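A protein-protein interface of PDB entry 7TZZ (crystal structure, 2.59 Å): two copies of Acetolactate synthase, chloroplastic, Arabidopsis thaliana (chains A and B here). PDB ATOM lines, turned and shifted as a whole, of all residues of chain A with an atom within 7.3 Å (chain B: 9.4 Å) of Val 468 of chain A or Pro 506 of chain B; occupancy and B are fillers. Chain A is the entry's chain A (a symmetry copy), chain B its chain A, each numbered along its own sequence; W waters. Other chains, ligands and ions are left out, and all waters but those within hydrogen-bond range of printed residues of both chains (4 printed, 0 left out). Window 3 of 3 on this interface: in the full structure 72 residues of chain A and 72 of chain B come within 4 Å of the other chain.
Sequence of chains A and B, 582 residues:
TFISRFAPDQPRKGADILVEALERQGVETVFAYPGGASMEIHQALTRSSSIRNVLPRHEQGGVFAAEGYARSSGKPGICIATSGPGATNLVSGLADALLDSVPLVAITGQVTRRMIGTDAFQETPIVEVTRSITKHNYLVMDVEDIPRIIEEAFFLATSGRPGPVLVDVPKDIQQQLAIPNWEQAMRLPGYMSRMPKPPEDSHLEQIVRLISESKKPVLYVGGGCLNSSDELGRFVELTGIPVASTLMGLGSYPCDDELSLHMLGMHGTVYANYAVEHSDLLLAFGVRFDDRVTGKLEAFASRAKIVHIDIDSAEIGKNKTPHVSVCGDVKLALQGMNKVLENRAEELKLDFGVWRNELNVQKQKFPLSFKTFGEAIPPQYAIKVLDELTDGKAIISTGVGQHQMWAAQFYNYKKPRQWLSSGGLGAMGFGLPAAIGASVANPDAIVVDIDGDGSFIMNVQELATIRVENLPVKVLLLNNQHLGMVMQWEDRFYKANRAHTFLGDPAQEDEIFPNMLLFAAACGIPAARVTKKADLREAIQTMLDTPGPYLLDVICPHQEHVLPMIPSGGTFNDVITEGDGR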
ATOM      1  N   ARG A  52     -23.347   3.286   4.480  1.00  0.00           N
ATOM      2  CA  ARG A  52     -22.709   4.529   4.874  1.00  0.00           C
ATOM      3  C   ARG A  52     -23.742   5.471   5.495  1.00  0.00           C
ATOM      4  O   ARG A  52     -24.867   5.577   5.000  1.00  0.00           O
ATOM      5  CB  ARG A  52     -22.045   5.178   3.661  1.00  0.00           C
ATOM      6  CG  ARG A  52     -21.745   6.665   3.777  1.00  0.00           C
ATOM      7  CD  ARG A  52     -21.496   7.297   2.392  1.00  0.00           C
ATOM      8  NE  ARG A  52     -20.877   8.625   2.485  1.00  0.00           N
ATOM      9  CZ  ARG A  52     -20.657   9.427   1.440  1.00  0.00           C
ATOM     10  NH1 ARG A  52     -21.006   9.040   0.205  1.00  0.00           N
ATOM     11  NH2 ARG A  52     -20.095  10.623   1.627  1.00  0.00           N
ATOM     12  N   VAL A  54     -24.541   9.451   6.301  1.00  0.00           N
ATOM     13  CA  VAL A  54     -24.222  10.863   6.133  1.00  0.00           C
ATOM     14  C   VAL A  54     -24.911  11.590   7.270  1.00  0.00           C
ATOM     15  O   VAL A  54     -26.146  11.702   7.288  1.00  0.00           O
ATOM     16  CB  VAL A  54     -24.667  11.409   4.777  1.00  0.00           C
ATOM     17  CG1 VAL A  54     -24.359  12.895   4.692  1.00  0.00           C
ATOM     18  CG2 VAL A  54     -24.005  10.637   3.640  1.00  0.00           C
ATOM     19  N   LEU A  55     -24.121  12.044   8.238  1.00  0.00           N
ATOM     20  CA  LEU A  55     -24.588  12.807   9.378  1.00  0.00           C
ATOM     21  C   LEU A  55     -24.943  14.241   8.993  1.00  0.00           C
ATOM     22  O   LEU A  55     -24.049  15.048   8.711  1.00  0.00           O
ATOM     23  CB  LEU A  55     -23.507  12.796  10.456  1.00  0.00           C
ATOM     24  CG  LEU A  55     -23.681  13.736  11.646  1.00  0.00           C
ATOM     25  CD1 LEU A  55     -24.836  13.228  12.503  1.00  0.00           C
ATOM     26  CD2 LEU A  55     -22.397  13.839  12.462  1.00  0.00           C
ATOM     27  N   ARG A  57     -26.694  18.115   9.937  1.00  0.00           N
ATOM     28  CA  ARG A  57     -26.577  18.950  11.116  1.00  0.00           C
ATOM     29  C   ARG A  57     -27.939  19.300  11.703  1.00  0.00           C
ATOM     30  O   ARG A  57     -28.014  19.976  12.739  1.00  0.00           O
ATOM     31  CB  ARG A  57     -25.777  20.214  10.788  1.00  0.00           C
ATOM     32  CG  ARG A  57     -24.332  20.128  11.227  1.00  0.00           C
ATOM     33  CD  ARG A  57     -23.664  18.968  10.540  1.00  0.00           C
ATOM     34  NE  ARG A  57     -22.277  18.799  10.971  1.00  0.00           N
ATOM     35  CZ  ARG A  57     -21.506  17.775  10.596  1.00  0.00           C
ATOM     36  NH1 ARG A  57     -21.991  16.823   9.791  1.00  0.00           N
ATOM     37  NH2 ARG A  57     -20.251  17.693  11.017  1.00  0.00           N
ATOM     38  N   GLU A 462     -26.242  22.935   6.930  1.00  0.00           N
ATOM     39  CA  GLU A 462     -25.788  21.796   6.142  1.00  0.00           C
ATOM     40  C   GLU A 462     -24.515  22.084   5.320  1.00  0.00           C
ATOM     41  O   GLU A 462     -23.971  21.161   4.691  1.00  0.00           O
ATOM     42  CB  GLU A 462     -26.942  21.326   5.236  1.00  0.00           C
ATOM     43  CG  GLU A 462     -28.194  20.956   6.002  1.00  0.00           C
ATOM     44  CD  GLU A 462     -27.925  19.995   7.183  1.00  0.00           C
ATOM     45  OE1 GLU A 462     -27.055  19.100   7.073  1.00  0.00           O
ATOM     46  OE2 GLU A 462     -28.587  20.128   8.224  1.00  0.00           O
ATOM     47  N   LEU A 463     -24.043  23.337   5.285  1.00  0.00           N
ATOM     48  CA  LEU A 463     -22.722  23.613   4.730  1.00  0.00           C
ATOM     49  C   LEU A 463     -21.646  22.782   5.419  1.00  0.00           C
ATOM     50  O   LEU A 463     -20.722  22.286   4.760  1.00  0.00           O
ATOM     51  CB  LEU A 463     -22.388  25.089   4.862  1.00  0.00           C
ATOM     52  CG  LEU A 463     -23.175  26.055   4.003  1.00  0.00           C
ATOM     53  CD1 LEU A 463     -22.731  27.459   4.337  1.00  0.00           C
ATOM     54  CD2 LEU A 463     -22.937  25.729   2.543  1.00  0.00           C
ATOM     55  N   ALA A 464     -21.774  22.599   6.743  1.00  0.00           N
ATOM     56  CA  ALA A 464     -20.862  21.737   7.487  1.00  0.00           C
ATOM     57  C   ALA A 464     -20.885  20.306   6.967  1.00  0.00           C
ATOM     58  O   ALA A 464     -19.835  19.668   6.826  1.00  0.00           O
ATOM     59  CB  ALA A 464     -21.219  21.773   8.966  1.00  0.00           C
ATOM     60  N   THR A 465     -22.078  19.785   6.683  1.00  0.00           N
ATOM     61  CA  THR A 465     -22.204  18.444   6.124  1.00  0.00           C
ATOM     62  C   THR A 465     -21.459  18.336   4.805  1.00  0.00           C
ATOM     63  O   THR A 465     -20.699  17.388   4.578  1.00  0.00           O
ATOM     64  CB  THR A 465     -23.685  18.114   5.908  1.00  0.00           C
ATOM     65  OG1 THR A 465     -24.401  18.302   7.136  1.00  0.00           O
ATOM     66  CG2 THR A 465     -23.881  16.661   5.391  1.00  0.00           C
ATOM     67  N   ILE A 466     -21.700  19.293   3.912  1.00  0.00           N
ATOM     68  CA  ILE A 466     -21.052  19.291   2.603  1.00  0.00           C
ATOM     69  C   ILE A 466     -19.531  19.227   2.748  1.00  0.00           C
ATOM     70  O   ILE A 466     -18.864  18.455   2.055  1.00  0.00           O
ATOM     71  CB  ILE A 466     -21.508  20.527   1.804  1.00  0.00           C
ATOM     72  CG1 ILE A 466     -22.925  20.288   1.276  1.00  0.00           C
ATOM     73  CG2 ILE A 466     -20.559  20.813   0.670  1.00  0.00           C
ATOM     74  CD1 ILE A 466     -23.761  21.529   1.024  1.00  0.00           C
ATOM     75  N   ARG A 467     -18.973  19.992   3.690  1.00  0.00           N
ATOM     76  CA  ARG A 467     -17.529  20.028   3.884  1.00  0.00           C
ATOM     77  C   ARG A 467     -16.986  18.690   4.374  1.00  0.00           C
ATOM     78  O   ARG A 467     -16.085  18.115   3.757  1.00  0.00           O
ATOM     79  CB  ARG A 467     -17.154  21.128   4.868  1.00  0.00           C
ATOM     80  CG  ARG A 467     -15.661  21.114   5.173  1.00  0.00           C
ATOM     81  CD  ARG A 467     -14.838  21.746   4.033  1.00  0.00           C
ATOM     82  NE  ARG A 467     -14.507  20.792   2.978  1.00  0.00           N
ATOM     83  CZ  ARG A 467     -14.106  21.124   1.746  1.00  0.00           C
ATOM     84  NH1 ARG A 467     -13.978  22.410   1.390  1.00  0.00           N
ATOM     85  NH2 ARG A 467     -13.834  20.168   0.854  1.00  0.00           N
ATOM     86  N   VAL A 468     -17.502  18.178   5.498  1.00  0.00           N
ATOM     87  CA  VAL A 468     -16.872  16.987   6.063  1.00  0.00           C
ATOM     88  C   VAL A 468     -17.132  15.778   5.188  1.00  0.00           C
ATOM     89  O   VAL A 468     -16.347  14.822   5.201  1.00  0.00           O
ATOM     90  CB  VAL A 468     -17.324  16.753   7.513  1.00  0.00           C
ATOM     91  CG1 VAL A 468     -17.153  18.019   8.293  1.00  0.00           C
ATOM     92  CG2 VAL A 468     -18.756  16.316   7.570  1.00  0.00           C
ATOM     93  N   GLU A 469     -18.216  15.795   4.398  1.00  0.00           N
ATOM     94  CA  GLU A 469     -18.488  14.690   3.494  1.00  0.00           C
ATOM     95  C   GLU A 469     -17.766  14.856   2.174  1.00  0.00           C
ATOM     96  O   GLU A 469     -17.856  13.958   1.314  1.00  0.00           O
ATOM     97  CB  GLU A 469     -19.994  14.557   3.233  1.00  0.00           C
ATOM     98  CG  GLU A 469     -20.809  14.212   4.459  1.00  0.00           C
ATOM     99  CD  GLU A 469     -20.475  12.826   5.012  1.00  0.00           C
ATOM    100  OE1 GLU A 469     -20.131  11.923   4.206  1.00  0.00           O
ATOM    101  OE2 GLU A 469     -20.578  12.628   6.246  1.00  0.00           O
ATOM    102  N   ASN A 470     -17.096  16.003   2.001  1.00  0.00           N
ATOM    103  CA  ASN A 470     -16.254  16.295   0.853  1.00  0.00           C
ATOM    104  C   ASN A 470     -17.037  16.078  -0.451  1.00  0.00           C
ATOM    105  O   ASN A 470     -16.588  15.438  -1.393  1.00  0.00           O
ATOM    106  CB  ASN A 470     -14.899  15.525   0.965  1.00  0.00           C
ATOM    107  CG  ASN A 470     -13.779  16.434   1.684  1.00  0.00           C
ATOM    108  OD1 ASN A 470     -13.309  17.413   1.102  1.00  0.00           O
ATOM    109  ND2 ASN A 470     -13.432  16.146   2.923  1.00  0.00           N
ATOM    110  N   LEU A 471     -18.256  16.684  -0.500  1.00  0.00           N
ATOM    111  CA  LEU A 471     -19.203  16.640  -1.611  1.00  0.00           C
ATOM    112  C   LEU A 471     -19.021  17.844  -2.528  1.00  0.00           C
ATOM    113  O   LEU A 471     -18.964  18.989  -2.051  1.00  0.00           O
ATOM    114  CB  LEU A 471     -20.644  16.621  -1.101  1.00  0.00           C
ATOM    115  CG  LEU A 471     -21.012  15.530  -0.103  1.00  0.00           C
ATOM    116  CD1 LEU A 471     -22.483  15.727   0.332  1.00  0.00           C
ATOM    117  CD2 LEU A 471     -20.783  14.155  -0.741  1.00  0.00           C
ATOM    118  N   CYS A 523     -17.325  27.136   7.128  1.00  0.00           N
ATOM    119  CA  CYS A 523     -17.334  25.698   6.885  1.00  0.00           C
ATOM    120  C   CYS A 523     -16.254  25.291   5.905  1.00  0.00           C
ATOM    121  O   CYS A 523     -16.303  24.182   5.366  1.00  0.00           O
ATOM    122  CB  CYS A 523     -18.709  25.240   6.378  1.00  0.00           C
ATOM    123  SG  CYS A 523     -20.040  25.430   7.641  1.00  0.00           S
ATOM    124  N   ILE A 525     -15.556  26.317   2.916  1.00  0.00           N
ATOM    125  CA  ILE A 525     -16.037  26.145   1.554  1.00  0.00           C
ATOM    126  C   ILE A 525     -15.639  27.386   0.762  1.00  0.00           C
ATOM    127  O   ILE A 525     -15.992  28.505   1.154  1.00  0.00           O
ATOM    128  CB  ILE A 525     -17.553  25.896   1.523  1.00  0.00           C
ATOM    129  CG1 ILE A 525     -17.851  24.508   2.119  1.00  0.00           C
ATOM    130  CG2 ILE A 525     -18.105  25.980   0.105  1.00  0.00           C
ATOM    131  CD1 ILE A 525     -19.356  24.243   2.339  1.00  0.00           C
ATOM    132  N   ILE B 457     -25.581  25.091  16.057  1.00  0.00           N
ATOM    133  CA  ILE B 457     -25.564  25.223  14.609  1.00  0.00           C
ATOM    134  C   ILE B 457     -26.947  24.962  14.034  1.00  0.00           C
ATOM    135  O   ILE B 457     -27.262  25.468  12.952  1.00  0.00           O
ATOM    136  CB  ILE B 457     -24.485  24.325  13.961  1.00  0.00           C
ATOM    137  CG1 ILE B 457     -24.106  24.888  12.582  1.00  0.00           C
ATOM    138  CG2 ILE B 457     -24.938  22.850  13.880  1.00  0.00           C
ATOM    139  CD1 ILE B 457     -23.055  24.053  11.841  1.00  0.00           C
ATOM    140  N   GLN B 481     -16.717  20.052  20.131  1.00  0.00           N
ATOM    141  CA  GLN B 481     -16.682  19.355  18.842  1.00  0.00           C
ATOM    142  C   GLN B 481     -17.468  18.040  18.823  1.00  0.00           C
ATOM    143  O   GLN B 481     -17.333  17.263  17.880  1.00  0.00           O
ATOM    144  CB  GLN B 481     -15.239  19.086  18.420  1.00  0.00           C
ATOM    145  CG  GLN B 481     -14.451  20.345  18.413  1.00  0.00           C
ATOM    146  CD  GLN B 481     -14.771  21.161  17.174  1.00  0.00           C
ATOM    147  OE1 GLN B 481     -14.213  20.921  16.101  1.00  0.00           O
ATOM    148  NE2 GLN B 481     -15.689  22.130  17.310  1.00  0.00           N
ATOM    149  N   HIS B 500     -21.161   8.423  15.001  1.00  0.00           N
ATOM    150  CA  HIS B 500     -21.609   9.683  14.396  1.00  0.00           C
ATOM    151  C   HIS B 500     -21.817  10.778  15.430  1.00  0.00           C
ATOM    152  O   HIS B 500     -22.725  11.589  15.292  1.00  0.00           O
ATOM    153  CB  HIS B 500     -22.880   9.458  13.569  1.00  0.00           C
ATOM    154  CG  HIS B 500     -22.850   8.158  12.828  1.00  0.00           C
ATOM    155  ND1 HIS B 500     -23.646   7.083  13.166  1.00  0.00           N
ATOM    156  CD2 HIS B 500     -22.048   7.733  11.820  1.00  0.00           C
ATOM    157  CE1 HIS B 500     -23.361   6.062  12.371  1.00  0.00           C
ATOM    158  NE2 HIS B 500     -22.394   6.430  11.547  1.00  0.00           N
ATOM    159  N   PHE B 502     -19.070  12.817  16.458  1.00  0.00           N
ATOM    160  CA  PHE B 502     -18.058  13.842  16.235  1.00  0.00           C
ATOM    161  C   PHE B 502     -18.573  14.858  15.230  1.00  0.00           C
ATOM    162  O   PHE B 502     -18.960  14.494  14.098  1.00  0.00           O
ATOM    163  CB  PHE B 502     -16.772  13.207  15.699  1.00  0.00           C
ATOM    164  CG  PHE B 502     -15.680  14.197  15.374  1.00  0.00           C
ATOM    165  CD1 PHE B 502     -15.200  15.082  16.349  1.00  0.00           C
ATOM    166  CD2 PHE B 502     -15.121  14.235  14.107  1.00  0.00           C
ATOM    167  CE1 PHE B 502     -14.193  16.001  16.039  1.00  0.00           C
ATOM    168  CE2 PHE B 502     -14.098  15.142  13.804  1.00  0.00           C
ATOM    169  CZ  PHE B 502     -13.627  16.017  14.766  1.00  0.00           C
ATOM    170  N   LEU B 503     -18.530  16.133  15.626  1.00  0.00           N
ATOM    171  CA  LEU B 503     -19.068  17.208  14.790  1.00  0.00           C
ATOM    172  C   LEU B 503     -18.025  17.965  13.968  1.00  0.00           C
ATOM    173  O   LEU B 503     -18.416  18.822  13.163  1.00  0.00           O
ATOM    174  CB  LEU B 503     -19.821  18.222  15.658  1.00  0.00           C
ATOM    175  CG  LEU B 503     -21.065  17.650  16.311  1.00  0.00           C
ATOM    176  CD1 LEU B 503     -21.496  18.663  17.283  1.00  0.00           C
ATOM    177  CD2 LEU B 503     -22.139  17.355  15.250  1.00  0.00           C
ATOM    178  N   GLY B 504     -16.724  17.725  14.189  1.00  0.00           N
ATOM    179  CA  GLY B 504     -15.689  18.453  13.477  1.00  0.00           C
ATOM    180  C   GLY B 504     -15.411  17.823  12.120  1.00  0.00           C
ATOM    181  O   GLY B 504     -16.151  16.966  11.636  1.00  0.00           O
ATOM    182  N   ASP B 505     -14.309  18.267  11.496  1.00  0.00           N
ATOM    183  CA  ASP B 505     -13.907  17.761  10.186  1.00  0.00           C
ATOM    184  C   ASP B 505     -12.880  16.657  10.376  1.00  0.00           C
ATOM    185  O   ASP B 505     -11.764  16.943  10.822  1.00  0.00           O
ATOM    186  CB  ASP B 505     -13.331  18.879   9.331  1.00  0.00           C
ATOM    187  CG  ASP B 505     -13.065  18.446   7.872  1.00  0.00           C
ATOM    188  OD1 ASP B 505     -13.129  17.226   7.578  1.00  0.00           O
ATOM    189  OD2 ASP B 505     -12.782  19.339   7.022  1.00  0.00           O
ATOM    190  N   PRO B 506     -13.191  15.399  10.055  1.00  0.00           N
ATOM    191  CA  PRO B 506     -12.214  14.329  10.301  1.00  0.00           C
ATOM    192  C   PRO B 506     -10.980  14.438   9.417  1.00  0.00           C
ATOM    193  O   PRO B 506      -9.945  13.849   9.747  1.00  0.00           O
ATOM    194  CB  PRO B 506     -13.007  13.044   9.994  1.00  0.00           C
ATOM    195  CG  PRO B 506     -14.410  13.470   9.794  1.00  0.00           C
ATOM    196  CD  PRO B 506     -14.360  14.889   9.332  1.00  0.00           C
ATOM    197  N   ALA B 507     -11.061  15.170   8.303  1.00  0.00           N
ATOM    198  CA  ALA B 507      -9.896  15.387   7.447  1.00  0.00           C
ATOM    199  C   ALA B 507      -8.840  16.259   8.119  1.00  0.00           C
ATOM    200  O   ALA B 507      -7.657  16.176   7.771  1.00  0.00           O
ATOM    201  CB  ALA B 507     -10.327  16.033   6.132  1.00  0.00           C
ATOM    202  N   GLN B 508      -9.243  17.119   9.053  1.00  0.00           N
ATOM    203  CA  GLN B 508      -8.343  17.986   9.797  1.00  0.00           C
ATOM    204  C   GLN B 508      -8.804  17.955  11.259  1.00  0.00           C
ATOM    205  O   GLN B 508      -9.247  18.961  11.813  1.00  0.00           O
ATOM    206  CB  GLN B 508      -8.357  19.405   9.228  1.00  0.00           C
ATOM    207  CG  GLN B 508      -9.766  19.870   8.898  1.00  0.00           C
ATOM    208  CD  GLN B 508      -9.818  21.184   8.126  1.00  0.00           C
ATOM    209  OE1 GLN B 508      -8.769  21.806   7.876  1.00  0.00           O
ATOM    210  NE2 GLN B 508     -11.058  21.623   7.742  1.00  0.00           N
ATOM    211  N   GLU B 509      -8.687  16.785  11.897  1.00  0.00           N
ATOM    212  CA  GLU B 509      -9.465  16.521  13.113  1.00  0.00           C
ATOM    213  C   GLU B 509      -9.059  17.377  14.315  1.00  0.00           C
ATOM    214  O   GLU B 509      -9.836  17.468  15.273  1.00  0.00           O
ATOM    215  CB  GLU B 509      -9.411  15.024  13.469  1.00  0.00           C
ATOM    216  CG  GLU B 509      -8.081  14.528  14.013  1.00  0.00           C
ATOM    217  CD  GLU B 509      -8.189  13.174  14.710  1.00  0.00           C
ATOM    218  OE1 GLU B 509      -8.643  12.201  14.075  1.00  0.00           O
ATOM    219  OE2 GLU B 509      -7.807  13.083  15.895  1.00  0.00           O
ATOM    220  N   ASP B 510      -7.907  18.042  14.289  1.00  0.00           N
ATOM    221  CA  ASP B 510      -7.533  18.886  15.414  1.00  0.00           C
ATOM    222  C   ASP B 510      -7.845  20.357  15.173  1.00  0.00           C
ATOM    223  O   ASP B 510      -7.492  21.205  15.995  1.00  0.00           O
ATOM    224  CB  ASP B 510      -6.062  18.665  15.768  1.00  0.00           C
ATOM    225  CG  ASP B 510      -5.871  17.436  16.644  1.00  0.00           C
ATOM    226  OD1 ASP B 510      -6.606  17.305  17.653  1.00  0.00           O
ATOM    227  OD2 ASP B 510      -5.029  16.580  16.303  1.00  0.00           O
ATOM    228  N   GLU B 511      -8.552  20.671  14.100  1.00  0.00           N
ATOM    229  CA  GLU B 511      -9.039  22.014  13.838  1.00  0.00           C
ATOM    230  C   GLU B 511     -10.459  22.179  14.374  1.00  0.00           C
ATOM    231  O   GLU B 511     -11.276  21.264  14.260  1.00  0.00           O
ATOM    232  CB  GLU B 511      -8.999  22.273  12.336  1.00  0.00           C
ATOM    233  CG  GLU B 511      -7.601  22.483  11.830  1.00  0.00           C
ATOM    234  CD  GLU B 511      -7.041  23.817  12.279  1.00  0.00           C
ATOM    235  OE1 GLU B 511      -7.764  24.837  12.172  1.00  0.00           O
ATOM    236  OE2 GLU B 511      -5.895  23.834  12.775  1.00  0.00           O
ATOM    237  N   ILE B 512     -10.743  23.335  14.974  1.00  0.00           N
ATOM    238  CA  ILE B 512     -12.094  23.637  15.445  1.00  0.00           C
ATOM    239  C   ILE B 512     -12.988  23.843  14.223  1.00  0.00           C
ATOM    240  O   ILE B 512     -12.838  24.829  13.494  1.00  0.00           O
ATOM    241  CB  ILE B 512     -12.120  24.870  16.352  1.00  0.00           C
ATOM    242  CG1 ILE B 512     -11.262  24.638  17.576  1.00  0.00           C
ATOM    243  CG2 ILE B 512     -13.570  25.173  16.802  1.00  0.00           C
ATOM    244  CD1 ILE B 512     -11.684  23.424  18.384  1.00  0.00           C
ATOM    245  N   PHE B 513     -13.939  22.933  14.021  1.00  0.00           N
ATOM    246  CA  PHE B 513     -14.829  22.960  12.867  1.00  0.00           C
ATOM    247  C   PHE B 513     -16.284  22.836  13.309  1.00  0.00           C
ATOM    248  O   PHE B 513     -16.622  21.942  14.105  1.00  0.00           O
ATOM    249  CB  PHE B 513     -14.505  21.838  11.866  1.00  0.00           C
ATOM    250  CG  PHE B 513     -15.344  21.904  10.643  1.00  0.00           C
ATOM    251  CD1 PHE B 513     -14.981  22.739   9.585  1.00  0.00           C
ATOM    252  CD2 PHE B 513     -16.547  21.183  10.566  1.00  0.00           C
ATOM    253  CE1 PHE B 513     -15.795  22.848   8.435  1.00  0.00           C
ATOM    254  CE2 PHE B 513     -17.357  21.269   9.438  1.00  0.00           C
ATOM    255  CZ  PHE B 513     -16.984  22.121   8.362  1.00  0.00           C
ATOM    256  N   PRO B 514     -17.181  23.675  12.798  1.00  0.00           N
ATOM    257  CA  PRO B 514     -16.883  24.823  11.955  1.00  0.00           C
ATOM    258  C   PRO B 514     -16.279  25.924  12.768  1.00  0.00           C
ATOM    259  O   PRO B 514     -16.128  25.808  13.980  1.00  0.00           O
ATOM    260  CB  PRO B 514     -18.267  25.246  11.433  1.00  0.00           C
ATOM    261  CG  PRO B 514     -19.139  24.059  11.661  1.00  0.00           C
ATOM    262  CD  PRO B 514     -18.629  23.441  12.893  1.00  0.00           C
HETATM  263  O   HOH W   1     -20.786  20.445  12.657  1.00  0.00           O
HETATM  264  O   HOH W   2     -18.489  15.368  11.482  1.00  0.00           O
HETATM  265  O   HOH W   3     -11.930  19.449   4.345  1.00  0.00           O
HETATM  266  O   HOH W   4     -13.720  15.385   5.802  1.00  0.00           O
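His 500 of chain B touches Leu 55 of chain A (O to CD2, 3.6 Å). CD2 of Leu 55 of chain A touches O of Phe 502 of chain B, at 3.9 Å. Ile 457 of chain B touches Arg 57 of chain A. CB of Ala 464 of chain A touches CE2 of Phe 513 of chain B, at 3.9 Å. CG of Arg 467 of chain A touches OD2 of Asp 505 of chain B (3.9 Å). Gly 504 of chain B touches Val 468 of chain A (O to CG1, 3.6 Å). CA of Asp 505 of chain B touches CG1 of Val 468 of chain A, 3.8 Å away. Pro 506 of chain B touches Val 468 of chain A. Phe 513 of chain B touches Val 468 of chain A (CE2 to CG1, 3.5 Å). O of Cys 523 of chain A touches CE1 of Phe 513 of chain B, 3.4 Å away.
The backbone carbonyl oxygen (O) of Leu 503 of chain B sits at hydrogen-bond distance from the guanidinium group (NH2) of Arg 57 of chain A (3.0 Å).
Of the 16 printed residues of chain A, 6 touch a printed residue of chain B. Of the 16 printed residues of chain B, 8 touch a printed residue of chain A. Hydrophobic or aromatic side chains of chain B within 4 Å of the printed part of chain A: Ile 457, Pro 506 and Phe 513.
Of chain B, only Gly 504 (3.6 Å), Asp 505 (3.8 Å), Pro 506 (3.9 Å) and Phe 513 (3.5 Å) come within 4 Å of Val 468 of chain A. Of chain A, only Val 468 (3.9 Å) comes within 4 Å of Pro 506 of chain B. Of the printed residues of chain B, Ala 464 of chain A touches Phe 513 (3.9 Å). Printed residues of chain A within 4 Å of Phe 513 of chain B: Ala 464 (3.9 Å), Arg 467 (3.6 Å), Val 468 (3.5 Å) and Cys 523 (3.4 Å). Of the printed residues of chain A, Phe 502 of chain B touches Leu 55. Printed residues of chain A within 4 Å of Leu 503 of chain B: Arg 57. Of the printed residues of chain B, Arg 467 of chain A touches Asp 505 and Phe 513. Arg 52 of chain A touches none of the printed residues of chain B. Glu 511 of chain B touches none of the printed residues of chain A. The nearest residue of chain B that does not touch Val 468 of chain A is Leu 503 of chain B (5.1 Å).
Water W4 lies within hydrogen-bond range of OD1 of Asp 505 of chain B (2.6 Å), O of Val 468 of chain A (2.8 Å) and ND2 of Asn 470 of chain A (3.0 Å). Water W1 bridges NE of Arg 57 of chain A and O of Leu 503 of chain B. Water W2 lies within hydrogen-bond range of O of Phe 502 of chain B (2.8 Å), O of Gly 504 of chain B (2.8 Å) and NH2 of Arg 57 of chain A (3.0 Å). Water W3 bridges OD2 of Asp 505 of chain B (2.8 Å) and NE of Arg 467 of chain A (3.2 Å).
No position is printed for both chains. Of the 12 pairs that touch across the chains among the printed residues, none has its exchanged pair printed and touching as well.
N of Ala 464 of chain A sits at hydrogen-bond distance from SG of Cys 523 of chain A (3.4 Å). The guanidinium group of Arg 467 of chain A sits at hydrogen-bond distance from the side-chain amide oxygen of Asn 470 of chain A (2.8 Å). The guanidinium group (NH1) of Arg 57 of chain A lies within hydrogen-bond range of the backbone carbonyl oxygen (O) of Leu 55 of chain A (2.9 Å). OE1 of Gln 481 of chain B sits at hydrogen-bond distance from N of Phe 513 of chain B, at 2.9 Å. The side-chain amide nitrogen (NE2) of Gln 508 of chain B is in hydrogen-bond range of the side-chain carboxylate (OD2) of Asp 505 of chain B, 3.0 Å away. The side-chain carboxylate (OD1) of Asp 505 of chain B is in hydrogen-bond range of the backbone NH (N) of Ala 507 of chain B (3.0 Å).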
